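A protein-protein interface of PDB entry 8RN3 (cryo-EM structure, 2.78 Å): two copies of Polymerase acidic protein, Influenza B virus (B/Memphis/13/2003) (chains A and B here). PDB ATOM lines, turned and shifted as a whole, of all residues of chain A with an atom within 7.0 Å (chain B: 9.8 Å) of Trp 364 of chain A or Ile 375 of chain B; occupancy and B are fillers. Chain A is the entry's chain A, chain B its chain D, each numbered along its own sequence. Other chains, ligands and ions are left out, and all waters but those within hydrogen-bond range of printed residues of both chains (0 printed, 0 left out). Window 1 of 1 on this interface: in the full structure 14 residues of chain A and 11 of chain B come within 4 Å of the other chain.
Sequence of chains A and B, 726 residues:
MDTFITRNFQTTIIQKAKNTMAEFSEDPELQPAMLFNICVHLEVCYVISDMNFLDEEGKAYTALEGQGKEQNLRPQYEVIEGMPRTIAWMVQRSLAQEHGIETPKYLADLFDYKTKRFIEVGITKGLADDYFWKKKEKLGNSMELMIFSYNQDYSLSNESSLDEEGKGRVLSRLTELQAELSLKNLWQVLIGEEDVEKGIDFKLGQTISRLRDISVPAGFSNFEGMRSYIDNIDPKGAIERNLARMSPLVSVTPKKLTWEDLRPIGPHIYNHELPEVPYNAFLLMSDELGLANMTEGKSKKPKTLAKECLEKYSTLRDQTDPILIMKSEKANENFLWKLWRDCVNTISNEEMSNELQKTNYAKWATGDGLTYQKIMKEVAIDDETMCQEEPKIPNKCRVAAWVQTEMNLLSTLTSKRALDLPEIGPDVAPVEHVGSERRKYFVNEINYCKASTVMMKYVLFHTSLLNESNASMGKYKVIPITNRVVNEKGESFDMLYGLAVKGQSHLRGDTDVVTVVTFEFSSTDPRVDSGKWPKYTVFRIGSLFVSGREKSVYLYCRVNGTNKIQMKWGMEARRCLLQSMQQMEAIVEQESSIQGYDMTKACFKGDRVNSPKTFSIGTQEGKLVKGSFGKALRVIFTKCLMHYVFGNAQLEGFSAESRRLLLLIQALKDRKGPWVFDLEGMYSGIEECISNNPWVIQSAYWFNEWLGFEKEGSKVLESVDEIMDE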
ATOM      1  N   PHE A 335     -20.494   6.434  21.363  1.00  0.00           N
ATOM      2  CA  PHE A 335     -21.253   7.284  22.272  1.00  0.00           C
ATOM      3  C   PHE A 335     -22.591   6.649  22.619  1.00  0.00           C
ATOM      4  O   PHE A 335     -22.988   6.606  23.788  1.00  0.00           O
ATOM      5  CB  PHE A 335     -21.478   8.660  21.641  1.00  0.00           C
ATOM      6  CG  PHE A 335     -20.255   9.541  21.609  1.00  0.00           C
ATOM      7  CD1 PHE A 335     -19.083   9.179  22.252  1.00  0.00           C
ATOM      8  CD2 PHE A 335     -20.287  10.744  20.927  1.00  0.00           C
ATOM      9  CE1 PHE A 335     -17.974   9.999  22.213  1.00  0.00           C
ATOM     10  CE2 PHE A 335     -19.182  11.566  20.887  1.00  0.00           C
ATOM     11  CZ  PHE A 335     -18.024  11.192  21.530  1.00  0.00           C
ATOM     12  N   LEU A 339     -23.811   5.316  26.260  1.00  0.00           N
ATOM     13  CA  LEU A 339     -25.022   5.861  26.866  1.00  0.00           C
ATOM     14  C   LEU A 339     -25.991   4.751  27.253  1.00  0.00           C
ATOM     15  O   LEU A 339     -26.598   4.792  28.328  1.00  0.00           O
ATOM     16  CB  LEU A 339     -25.696   6.836  25.904  1.00  0.00           C
ATOM     17  CG  LEU A 339     -25.425   8.327  26.098  1.00  0.00           C
ATOM     18  CD1 LEU A 339     -26.226   9.123  25.086  1.00  0.00           C
ATOM     19  CD2 LEU A 339     -25.758   8.777  27.509  1.00  0.00           C
ATOM     20  N   THR A 359     -22.233  11.809  33.928  1.00  0.00           N
ATOM     21  CA  THR A 359     -22.862  13.000  33.368  1.00  0.00           C
ATOM     22  C   THR A 359     -21.915  13.733  32.428  1.00  0.00           C
ATOM     23  O   THR A 359     -22.339  14.242  31.383  1.00  0.00           O
ATOM     24  CB  THR A 359     -23.326  13.921  34.496  1.00  0.00           C
ATOM     25  OG1 THR A 359     -24.562  13.434  35.034  1.00  0.00           O
ATOM     26  CG2 THR A 359     -23.523  15.346  33.992  1.00  0.00           C
ATOM     27  N   ASN A 360     -20.630  13.799  32.777  1.00  0.00           N
ATOM     28  CA  ASN A 360     -19.671  14.485  31.917  1.00  0.00           C
ATOM     29  C   ASN A 360     -19.571  13.805  30.559  1.00  0.00           C
ATOM     30  O   ASN A 360     -19.518  14.478  29.524  1.00  0.00           O
ATOM     31  CB  ASN A 360     -18.303  14.535  32.595  1.00  0.00           C
ATOM     32  CG  ASN A 360     -18.293  15.422  33.823  1.00  0.00           C
ATOM     33  OD1 ASN A 360     -19.131  16.312  33.966  1.00  0.00           O
ATOM     34  ND2 ASN A 360     -17.342  15.184  34.717  1.00  0.00           N
ATOM     35  N   TYR A 361     -19.536  12.472  30.541  1.00  0.00           N
ATOM     36  CA  TYR A 361     -19.517  11.757  29.271  1.00  0.00           C
ATOM     37  C   TYR A 361     -20.840  11.912  28.534  1.00  0.00           C
ATOM     38  O   TYR A 361     -20.856  12.130  27.318  1.00  0.00           O
ATOM     39  CB  TYR A 361     -19.205  10.280  29.501  1.00  0.00           C
ATOM     40  CG  TYR A 361     -19.044   9.494  28.222  1.00  0.00           C
ATOM     41  CD1 TYR A 361     -20.139   8.923  27.590  1.00  0.00           C
ATOM     42  CD2 TYR A 361     -17.795   9.326  27.642  1.00  0.00           C
ATOM     43  CE1 TYR A 361     -19.996   8.209  26.421  1.00  0.00           C
ATOM     44  CE2 TYR A 361     -17.643   8.614  26.473  1.00  0.00           C
ATOM     45  CZ  TYR A 361     -18.746   8.059  25.867  1.00  0.00           C
ATOM     46  OH  TYR A 361     -18.595   7.348  24.703  1.00  0.00           O
ATOM     47  N   ALA A 362     -21.959  11.800  29.252  1.00  0.00           N
ATOM     48  CA  ALA A 362     -23.267  11.930  28.622  1.00  0.00           C
ATOM     49  C   ALA A 362     -23.479  13.312  28.028  1.00  0.00           C
ATOM     50  O   ALA A 362     -24.327  13.473  27.145  1.00  0.00           O
ATOM     51  CB  ALA A 362     -24.370  11.626  29.634  1.00  0.00           C
ATOM     52  N   LYS A 363     -22.733  14.315  28.495  1.00  0.00           N
ATOM     53  CA  LYS A 363     -22.841  15.645  27.907  1.00  0.00           C
ATOM     54  C   LYS A 363     -22.445  15.625  26.437  1.00  0.00           C
ATOM     55  O   LYS A 363     -23.082  16.281  25.605  1.00  0.00           O
ATOM     56  CB  LYS A 363     -21.966  16.629  28.683  1.00  0.00           C
ATOM     57  CG  LYS A 363     -22.045  18.066  28.189  1.00  0.00           C
ATOM     58  CD  LYS A 363     -20.817  18.858  28.592  1.00  0.00           C
ATOM     59  CE  LYS A 363     -20.781  20.208  27.906  1.00  0.00           C
ATOM     60  NZ  LYS A 363     -19.660  21.053  28.397  1.00  0.00           N
ATOM     61  N   TRP A 364     -21.392  14.885  26.100  1.00  0.00           N
ATOM     62  CA  TRP A 364     -20.907  14.819  24.729  1.00  0.00           C
ATOM     63  C   TRP A 364     -21.509  13.660  23.951  1.00  0.00           C
ATOM     64  O   TRP A 364     -21.659  13.756  22.728  1.00  0.00           O
ATOM     65  CB  TRP A 364     -19.383  14.702  24.728  1.00  0.00           C
ATOM     66  CG  TRP A 364     -18.710  15.930  25.246  1.00  0.00           C
ATOM     67  CD1 TRP A 364     -18.059  16.067  26.436  1.00  0.00           C
ATOM     68  CD2 TRP A 364     -18.623  17.199  24.591  1.00  0.00           C
ATOM     69  NE1 TRP A 364     -17.575  17.345  26.564  1.00  0.00           N
ATOM     70  CE2 TRP A 364     -17.907  18.060  25.443  1.00  0.00           C
ATOM     71  CE3 TRP A 364     -19.082  17.692  23.366  1.00  0.00           C
ATOM     72  CZ2 TRP A 364     -17.637  19.385  25.110  1.00  0.00           C
ATOM     73  CZ3 TRP A 364     -18.813  19.005  23.038  1.00  0.00           C
ATOM     74  CH2 TRP A 364     -18.098  19.836  23.906  1.00  0.00           C
ATOM     75  N   ALA A 365     -21.859  12.568  24.631  1.00  0.00           N
ATOM     76  CA  ALA A 365     -22.484  11.444  23.948  1.00  0.00           C
ATOM     77  C   ALA A 365     -23.825  11.835  23.344  1.00  0.00           C
ATOM     78  O   ALA A 365     -24.205  11.316  22.289  1.00  0.00           O
ATOM     79  CB  ALA A 365     -22.659  10.277  24.917  1.00  0.00           C
ATOM     80  N   THR A 366     -24.553  12.739  23.996  1.00  0.00           N
ATOM     81  CA  THR A 366     -25.837  13.208  23.497  1.00  0.00           C
ATOM     82  C   THR A 366     -25.707  14.375  22.530  1.00  0.00           C
ATOM     83  O   THR A 366     -26.716  14.799  21.958  1.00  0.00           O
ATOM     84  CB  THR A 366     -26.736  13.630  24.664  1.00  0.00           C
ATOM     85  OG1 THR A 366     -26.139  14.730  25.358  1.00  0.00           O
ATOM     86  CG2 THR A 366     -26.939  12.479  25.634  1.00  0.00           C
ATOM     87  N   GLY A 367     -24.501  14.902  22.334  1.00  0.00           N
ATOM     88  CA  GLY A 367     -24.303  16.053  21.480  1.00  0.00           C
ATOM     89  C   GLY A 367     -24.661  17.377  22.111  1.00  0.00           C
ATOM     90  O   GLY A 367     -24.665  18.395  21.413  1.00  0.00           O
ATOM     91  N   ASP A 368     -24.960  17.399  23.411  1.00  0.00           N
ATOM     92  CA  ASP A 368     -25.380  18.637  24.055  1.00  0.00           C
ATOM     93  C   ASP A 368     -24.242  19.643  24.147  1.00  0.00           C
ATOM     94  O   ASP A 368     -24.490  20.854  24.188  1.00  0.00           O
ATOM     95  CB  ASP A 368     -25.932  18.340  25.448  1.00  0.00           C
ATOM     96  CG  ASP A 368     -27.388  17.931  25.425  1.00  0.00           C
ATOM     97  OD1 ASP A 368     -28.000  17.963  24.338  1.00  0.00           O
ATOM     98  OD2 ASP A 368     -27.923  17.579  26.496  1.00  0.00           O
ATOM     99  N   GLY A 369     -22.997  19.171  24.187  1.00  0.00           N
ATOM    100  CA  GLY A 369     -21.866  20.073  24.274  1.00  0.00           C
ATOM    101  C   GLY A 369     -21.540  20.795  22.985  1.00  0.00           C
ATOM    102  O   GLY A 369     -20.788  21.774  23.020  1.00  0.00           O
ATOM    103  N   LEU A 370     -22.081  20.342  21.859  1.00  0.00           N
ATOM    104  CA  LEU A 370     -21.815  20.957  20.560  1.00  0.00           C
ATOM    105  C   LEU A 370     -22.852  22.024  20.224  1.00  0.00           C
ATOM    106  O   LEU A 370     -23.456  22.018  19.153  1.00  0.00           O
ATOM    107  CB  LEU A 370     -21.777  19.880  19.482  1.00  0.00           C
ATOM    108  CG  LEU A 370     -20.539  18.985  19.407  1.00  0.00           C
ATOM    109  CD1 LEU A 370     -20.605  18.139  18.152  1.00  0.00           C
ATOM    110  CD2 LEU A 370     -19.254  19.796  19.427  1.00  0.00           C
ATOM    111  N   THR A 371     -23.059  22.960  21.143  1.00  0.00           N
ATOM    112  CA  THR A 371     -24.008  24.049  20.964  1.00  0.00           C
ATOM    113  C   THR A 371     -23.241  25.345  20.757  1.00  0.00           C
ATOM    114  O   THR A 371     -22.298  25.638  21.500  1.00  0.00           O
ATOM    115  CB  THR A 371     -24.940  24.172  22.171  1.00  0.00           C
ATOM    116  OG1 THR A 371     -25.652  22.942  22.357  1.00  0.00           O
ATOM    117  CG2 THR A 371     -25.938  25.302  21.964  1.00  0.00           C
ATOM    118  N   TYR A 476     -28.993  14.527  33.601  1.00  0.00           N
ATOM    119  CA  TYR A 476     -29.332  13.450  32.679  1.00  0.00           C
ATOM    120  C   TYR A 476     -30.011  12.327  33.451  1.00  0.00           C
ATOM    121  O   TYR A 476     -29.425  11.763  34.379  1.00  0.00           O
ATOM    122  CB  TYR A 476     -28.086  12.938  31.959  1.00  0.00           C
ATOM    123  CG  TYR A 476     -27.524  13.936  30.975  1.00  0.00           C
ATOM    124  CD1 TYR A 476     -28.152  14.166  29.761  1.00  0.00           C
ATOM    125  CD2 TYR A 476     -26.376  14.656  31.263  1.00  0.00           C
ATOM    126  CE1 TYR A 476     -27.651  15.080  28.863  1.00  0.00           C
ATOM    127  CE2 TYR A 476     -25.867  15.572  30.369  1.00  0.00           C
ATOM    128  CZ  TYR A 476     -26.510  15.779  29.170  1.00  0.00           C
ATOM    129  OH  TYR A 476     -26.010  16.690  28.272  1.00  0.00           O
ATOM    130  N   TYR B 372     -10.042  26.570  21.391  1.00  0.00           N
ATOM    131  CA  TYR B 372     -10.650  25.250  21.478  1.00  0.00           C
ATOM    132  C   TYR B 372     -10.800  24.836  22.936  1.00  0.00           C
ATOM    133  O   TYR B 372      -9.900  25.043  23.753  1.00  0.00           O
ATOM    134  CB  TYR B 372      -9.800  24.230  20.720  1.00  0.00           C
ATOM    135  CG  TYR B 372      -9.844  24.372  19.212  1.00  0.00           C
ATOM    136  CD1 TYR B 372     -10.404  25.492  18.609  1.00  0.00           C
ATOM    137  CD2 TYR B 372      -9.308  23.390  18.390  1.00  0.00           C
ATOM    138  CE1 TYR B 372     -10.440  25.622  17.236  1.00  0.00           C
ATOM    139  CE2 TYR B 372      -9.340  23.515  17.015  1.00  0.00           C
ATOM    140  CZ  TYR B 372      -9.905  24.632  16.445  1.00  0.00           C
ATOM    141  OH  TYR B 372      -9.937  24.758  15.076  1.00  0.00           O
ATOM    142  N   GLN B 373     -11.946  24.247  23.260  1.00  0.00           N
ATOM    143  CA  GLN B 373     -12.279  23.887  24.632  1.00  0.00           C
ATOM    144  C   GLN B 373     -11.895  22.436  24.892  1.00  0.00           C
ATOM    145  O   GLN B 373     -12.240  21.545  24.109  1.00  0.00           O
ATOM    146  CB  GLN B 373     -13.770  24.113  24.902  1.00  0.00           C
ATOM    147  CG  GLN B 373     -14.693  22.999  24.433  1.00  0.00           C
ATOM    148  CD  GLN B 373     -16.155  23.326  24.667  1.00  0.00           C
ATOM    149  OE1 GLN B 373     -16.718  22.992  25.708  1.00  0.00           O
ATOM    150  NE2 GLN B 373     -16.777  23.983  23.695  1.00  0.00           N
ATOM    151  N   LYS B 374     -11.176  22.209  25.988  1.00  0.00           N
ATOM    152  CA  LYS B 374     -10.732  20.868  26.336  1.00  0.00           C
ATOM    153  C   LYS B 374     -11.906  20.006  26.784  1.00  0.00           C
ATOM    154  O   LYS B 374     -12.873  20.489  27.378  1.00  0.00           O
ATOM    155  CB  LYS B 374      -9.682  20.922  27.444  1.00  0.00           C
ATOM    156  CG  LYS B 374      -9.106  19.564  27.808  1.00  0.00           C
ATOM    157  CD  LYS B 374      -7.766  19.689  28.512  1.00  0.00           C
ATOM    158  CE  LYS B 374      -6.618  19.804  27.523  1.00  0.00           C
ATOM    159  NZ  LYS B 374      -5.316  19.435  28.144  1.00  0.00           N
ATOM    160  N   ILE B 375     -11.810  18.709  26.490  1.00  0.00           N
ATOM    161  CA  ILE B 375     -12.818  17.735  26.877  1.00  0.00           C
ATOM    162  C   ILE B 375     -12.116  16.514  27.458  1.00  0.00           C
ATOM    163  O   ILE B 375     -10.920  16.297  27.250  1.00  0.00           O
ATOM    164  CB  ILE B 375     -13.726  17.330  25.695  1.00  0.00           C
ATOM    165  CG1 ILE B 375     -12.897  16.723  24.561  1.00  0.00           C
ATOM    166  CG2 ILE B 375     -14.504  18.534  25.196  1.00  0.00           C
ATOM    167  CD1 ILE B 375     -13.719  16.319  23.358  1.00  0.00           C
ATOM    168  N   MET B 376     -12.881  15.716  28.197  1.00  0.00           N
ATOM    169  CA  MET B 376     -12.322  14.531  28.833  1.00  0.00           C
ATOM    170  C   MET B 376     -11.775  13.575  27.777  1.00  0.00           C
ATOM    171  O   MET B 376     -12.315  13.452  26.677  1.00  0.00           O
ATOM    172  CB  MET B 376     -13.375  13.817  29.692  1.00  0.00           C
ATOM    173  CG  MET B 376     -14.804  13.831  29.144  1.00  0.00           C
ATOM    174  SD  MET B 376     -16.020  13.075  30.247  1.00  0.00           S
ATOM    175  CE  MET B 376     -15.183  11.579  30.752  1.00  0.00           C
ATOM    176  N   LYS B 377     -10.676  12.901  28.123  1.00  0.00           N
ATOM    177  CA  LYS B 377     -10.003  12.038  27.158  1.00  0.00           C
ATOM    178  C   LYS B 377     -10.878  10.876  26.705  1.00  0.00           C
ATOM    179  O   LYS B 377     -10.632  10.314  25.634  1.00  0.00           O
ATOM    180  CB  LYS B 377      -8.700  11.504  27.753  1.00  0.00           C
ATOM    181  CG  LYS B 377      -8.863  10.250  28.596  1.00  0.00           C
ATOM    182  CD  LYS B 377      -7.643  10.011  29.471  1.00  0.00           C
ATOM    183  CE  LYS B 377      -7.763   8.721  30.269  1.00  0.00           C
ATOM    184  NZ  LYS B 377      -8.116   7.550  29.419  1.00  0.00           N
ATOM    185  N   GLU B 378     -11.891  10.503  27.489  1.00  0.00           N
ATOM    186  CA  GLU B 378     -12.739   9.375  27.114  1.00  0.00           C
ATOM    187  C   GLU B 378     -13.539   9.685  25.852  1.00  0.00           C
ATOM    188  O   GLU B 378     -13.543   8.899  24.897  1.00  0.00           O
ATOM    189  CB  GLU B 378     -13.670   9.020  28.273  1.00  0.00           C
ATOM    190  CG  GLU B 378     -14.491   7.760  28.057  1.00  0.00           C
ATOM    191  CD  GLU B 378     -15.359   7.421  29.255  1.00  0.00           C
ATOM    192  OE1 GLU B 378     -15.326   8.178  30.248  1.00  0.00           O
ATOM    193  OE2 GLU B 378     -16.074   6.399  29.204  1.00  0.00           O
ATOM    194  N   VAL B 379     -14.221  10.833  25.828  1.00  0.00           N
ATOM    195  CA  VAL B 379     -14.993  11.198  24.644  1.00  0.00           C
ATOM    196  C   VAL B 379     -14.069  11.460  23.465  1.00  0.00           C
ATOM    197  O   VAL B 379     -14.412  11.151  22.319  1.00  0.00           O
ATOM    198  CB  VAL B 379     -15.895  12.413  24.937  1.00  0.00           C
ATOM    199  CG1 VAL B 379     -16.845  12.107  26.082  1.00  0.00           C
ATOM    200  CG2 VAL B 379     -15.065  13.645  25.254  1.00  0.00           C
ATOM    201  N   ALA B 380     -12.890  12.034  23.716  1.00  0.00           N
ATOM    202  CA  ALA B 380     -11.938  12.262  22.635  1.00  0.00           C
ATOM    203  C   ALA B 380     -11.503  10.946  22.006  1.00  0.00           C
ATOM    204  O   ALA B 380     -11.398  10.841  20.779  1.00  0.00           O
ATOM    205  CB  ALA B 380     -10.728  13.032  23.160  1.00  0.00           C
ATOM    206  N   ILE B 381     -11.240   9.932  22.832  1.00  0.00           N
ATOM    207  CA  ILE B 381     -10.878   8.619  22.309  1.00  0.00           C
ATOM    208  C   ILE B 381     -12.045   8.017  21.538  1.00  0.00           C
ATOM    209  O   ILE B 381     -11.866   7.452  20.454  1.00  0.00           O
ATOM    210  CB  ILE B 381     -10.420   7.700  23.457  1.00  0.00           C
ATOM    211  CG1 ILE B 381      -8.919   7.864  23.704  1.00  0.00           C
ATOM    212  CG2 ILE B 381     -10.739   6.241  23.145  1.00  0.00           C
ATOM    213  CD1 ILE B 381      -8.491   7.523  25.116  1.00  0.00           C
ATOM    214  N   ASP B 382     -13.259   8.124  22.084  1.00  0.00           N
ATOM    215  CA  ASP B 382     -14.419   7.554  21.410  1.00  0.00           C
ATOM    216  C   ASP B 382     -14.714   8.261  20.095  1.00  0.00           C
ATOM    217  O   ASP B 382     -15.264   7.648  19.174  1.00  0.00           O
ATOM    218  CB  ASP B 382     -15.642   7.619  22.323  1.00  0.00           C
ATOM    219  CG  ASP B 382     -15.782   6.393  23.198  1.00  0.00           C
ATOM    220  OD1 ASP B 382     -14.812   5.617  23.303  1.00  0.00           O
ATOM    221  OD2 ASP B 382     -16.868   6.208  23.782  1.00  0.00           O
ATOM    222  N   ASP B 383     -14.369   9.541  19.988  1.00  0.00           N
ATOM    223  CA  ASP B 383     -14.658  10.314  18.787  1.00  0.00           C
ATOM    224  C   ASP B 383     -13.598  10.035  17.730  1.00  0.00           C
ATOM    225  O   ASP B 383     -12.410  10.295  17.948  1.00  0.00           O
ATOM    226  CB  ASP B 383     -14.711  11.803  19.120  1.00  0.00           C
ATOM    227  CG  ASP B 383     -15.539  12.597  18.126  1.00  0.00           C
ATOM    228  OD1 ASP B 383     -16.339  11.986  17.388  1.00  0.00           O
ATOM    229  OD2 ASP B 383     -15.386  13.835  18.084  1.00  0.00           O
ATOM    230  N   GLU B 384     -14.027   9.506  16.583  1.00  0.00           N
ATOM    231  CA  GLU B 384     -13.110   9.173  15.500  1.00  0.00           C
ATOM    232  C   GLU B 384     -12.710  10.381  14.666  1.00  0.00           C
ATOM    233  O   GLU B 384     -11.765  10.280  13.875  1.00  0.00           O
ATOM    234  CB  GLU B 384     -13.740   8.117  14.589  1.00  0.00           C
ATOM    235  CG  GLU B 384     -14.019   6.792  15.277  1.00  0.00           C
ATOM    236  CD  GLU B 384     -15.355   6.774  15.993  1.00  0.00           C
ATOM    237  OE1 GLU B 384     -16.040   7.817  16.007  1.00  0.00           O
ATOM    238  OE2 GLU B 384     -15.721   5.712  16.541  1.00  0.00           O
ATOM    239  N   THR B 385     -13.394  11.510  14.819  1.00  0.00           N
ATOM    240  CA  THR B 385     -13.098  12.711  14.049  1.00  0.00           C
ATOM    241  C   THR B 385     -12.078  13.614  14.729  1.00  0.00           C
ATOM    242  O   THR B 385     -11.755  14.675  14.186  1.00  0.00           O
ATOM    243  CB  THR B 385     -14.385  13.503  13.788  1.00  0.00           C
ATOM    244  OG1 THR B 385     -14.646  14.376  14.894  1.00  0.00           O
ATOM    245  CG2 THR B 385     -15.569  12.565  13.585  1.00  0.00           C
ATOM    246  N   MET B 386     -11.565  13.225  15.895  1.00  0.00           N
ATOM    247  CA  MET B 386     -10.551  13.994  16.607  1.00  0.00           C
ATOM    248  C   MET B 386      -9.186  13.405  16.269  1.00  0.00           C
ATOM    249  O   MET B 386      -8.846  12.306  16.721  1.00  0.00           O
ATOM    250  CB  MET B 386     -10.809  13.971  18.112  1.00  0.00           C
ATOM    251  CG  MET B 386     -12.134  14.624  18.510  1.00  0.00           C
ATOM    252  SD  MET B 386     -12.254  15.365  20.158  1.00  0.00           S
ATOM    253  CE  MET B 386     -10.586  15.930  20.487  1.00  0.00           C
ATOM    254  N   CYS B 387      -8.407  14.138  15.477  1.00  0.00           N
ATOM    255  CA  CYS B 387      -7.113  13.679  14.998  1.00  0.00           C
ATOM    256  C   CYS B 387      -6.053  14.726  15.307  1.00  0.00           C
ATOM    257  O   CYS B 387      -6.345  15.914  15.456  1.00  0.00           O
ATOM    258  CB  CYS B 387      -7.141  13.399  13.489  1.00  0.00           C
ATOM    259  SG  CYS B 387      -8.334  12.135  12.985  1.00  0.00           S
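The backbone NH (N) of Tyr 361 of chain A is in hydrogen-bond range of the side-chain sulfur (SD) of Met 376 of chain B, 3.6 Å away. OD2 of Asp 382 of chain B sits close to OH of Tyr 361 of chain A, 2.3 Å away.
CZ of Phe 335 of chain A touches O of Val 379 of chain B (3.7 Å). CE1 of Phe 335 of chain A touches CB of Asp 382 of chain B, 3.3 Å away. CB of Asn 360 of chain A touches SD of Met 376 of chain B, 3.6 Å away. Tyr 361 of chain A touches Glu 378 of chain B. CD2 of Tyr 361 of chain A touches CG1 of Val 379 of chain B, at 3.3 Å. Gln 373 of chain B touches Trp 364 of chain A (OE1 to CZ2, 3.8 Å). Trp 364 of chain A touches Ile 375 of chain B (CZ2 to CG2, 3.2 Å). Trp 364 of chain A touches Val 379 of chain B.
Of chain B, only Gln 373, Ile 375 and Val 379 come within 4 Å of Trp 364 of chain A. Of chain A, only Trp 364 (3.2 Å) comes within 4 Å of Ile 375 of chain B. No residue of chain B comes within 4 Å of Ala 362 of chain A. No residue of chain B comes within 4 Å of Ala 365 of chain A. No residue of chain B comes within 4 Å of Gly 367 of chain A. No residue of chain B comes within 4 Å of Gly 369 of chain A. Printed residues of chain B within 4 Å of Tyr 361 of chain A: Met 376 (3.6 Å), Glu 378 (3.5 Å), Val 379 (3.3 Å) and Asp 382 (2.3 Å). Of the printed residues of chain A, Met 376 of chain B touches Asn 360 and Tyr 361. Of the printed residues of chain B, Asn 360 of chain A touches Met 376 (3.6 Å). The nearest residue of chain B that does not touch Trp 364 of chain A is Met 376 of chain B (4.8 Å). The nearest residue of chain A that does not touch Ile 375 of chain B is Lys 363 of chain A (6.6 Å). The nearest printed residue of chain A that does not touch Asp 382 of chain B is Ala 365 of chain A (7.2 Å).
Printed residues of chain B that touch a printed residue of chain A: Gln 373, Ile 375, Met 376, Glu 378, Val 379 and Asp 382. Of the 16 printed residues of chain A, 4 touch a printed residue of chain B. Hydrophobic or aromatic side chains of chain A within 4 Å of the printed part of chain B: Phe 335, Tyr 361 and Trp 364. Among the printed residues, 10 pairs touch across the chains. Among the printed residues, no Asp or Glu carboxylate lies within 4 Å of a Lys or Arg side-chain nitrogen of the other chain.
No position is printed for both chains.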
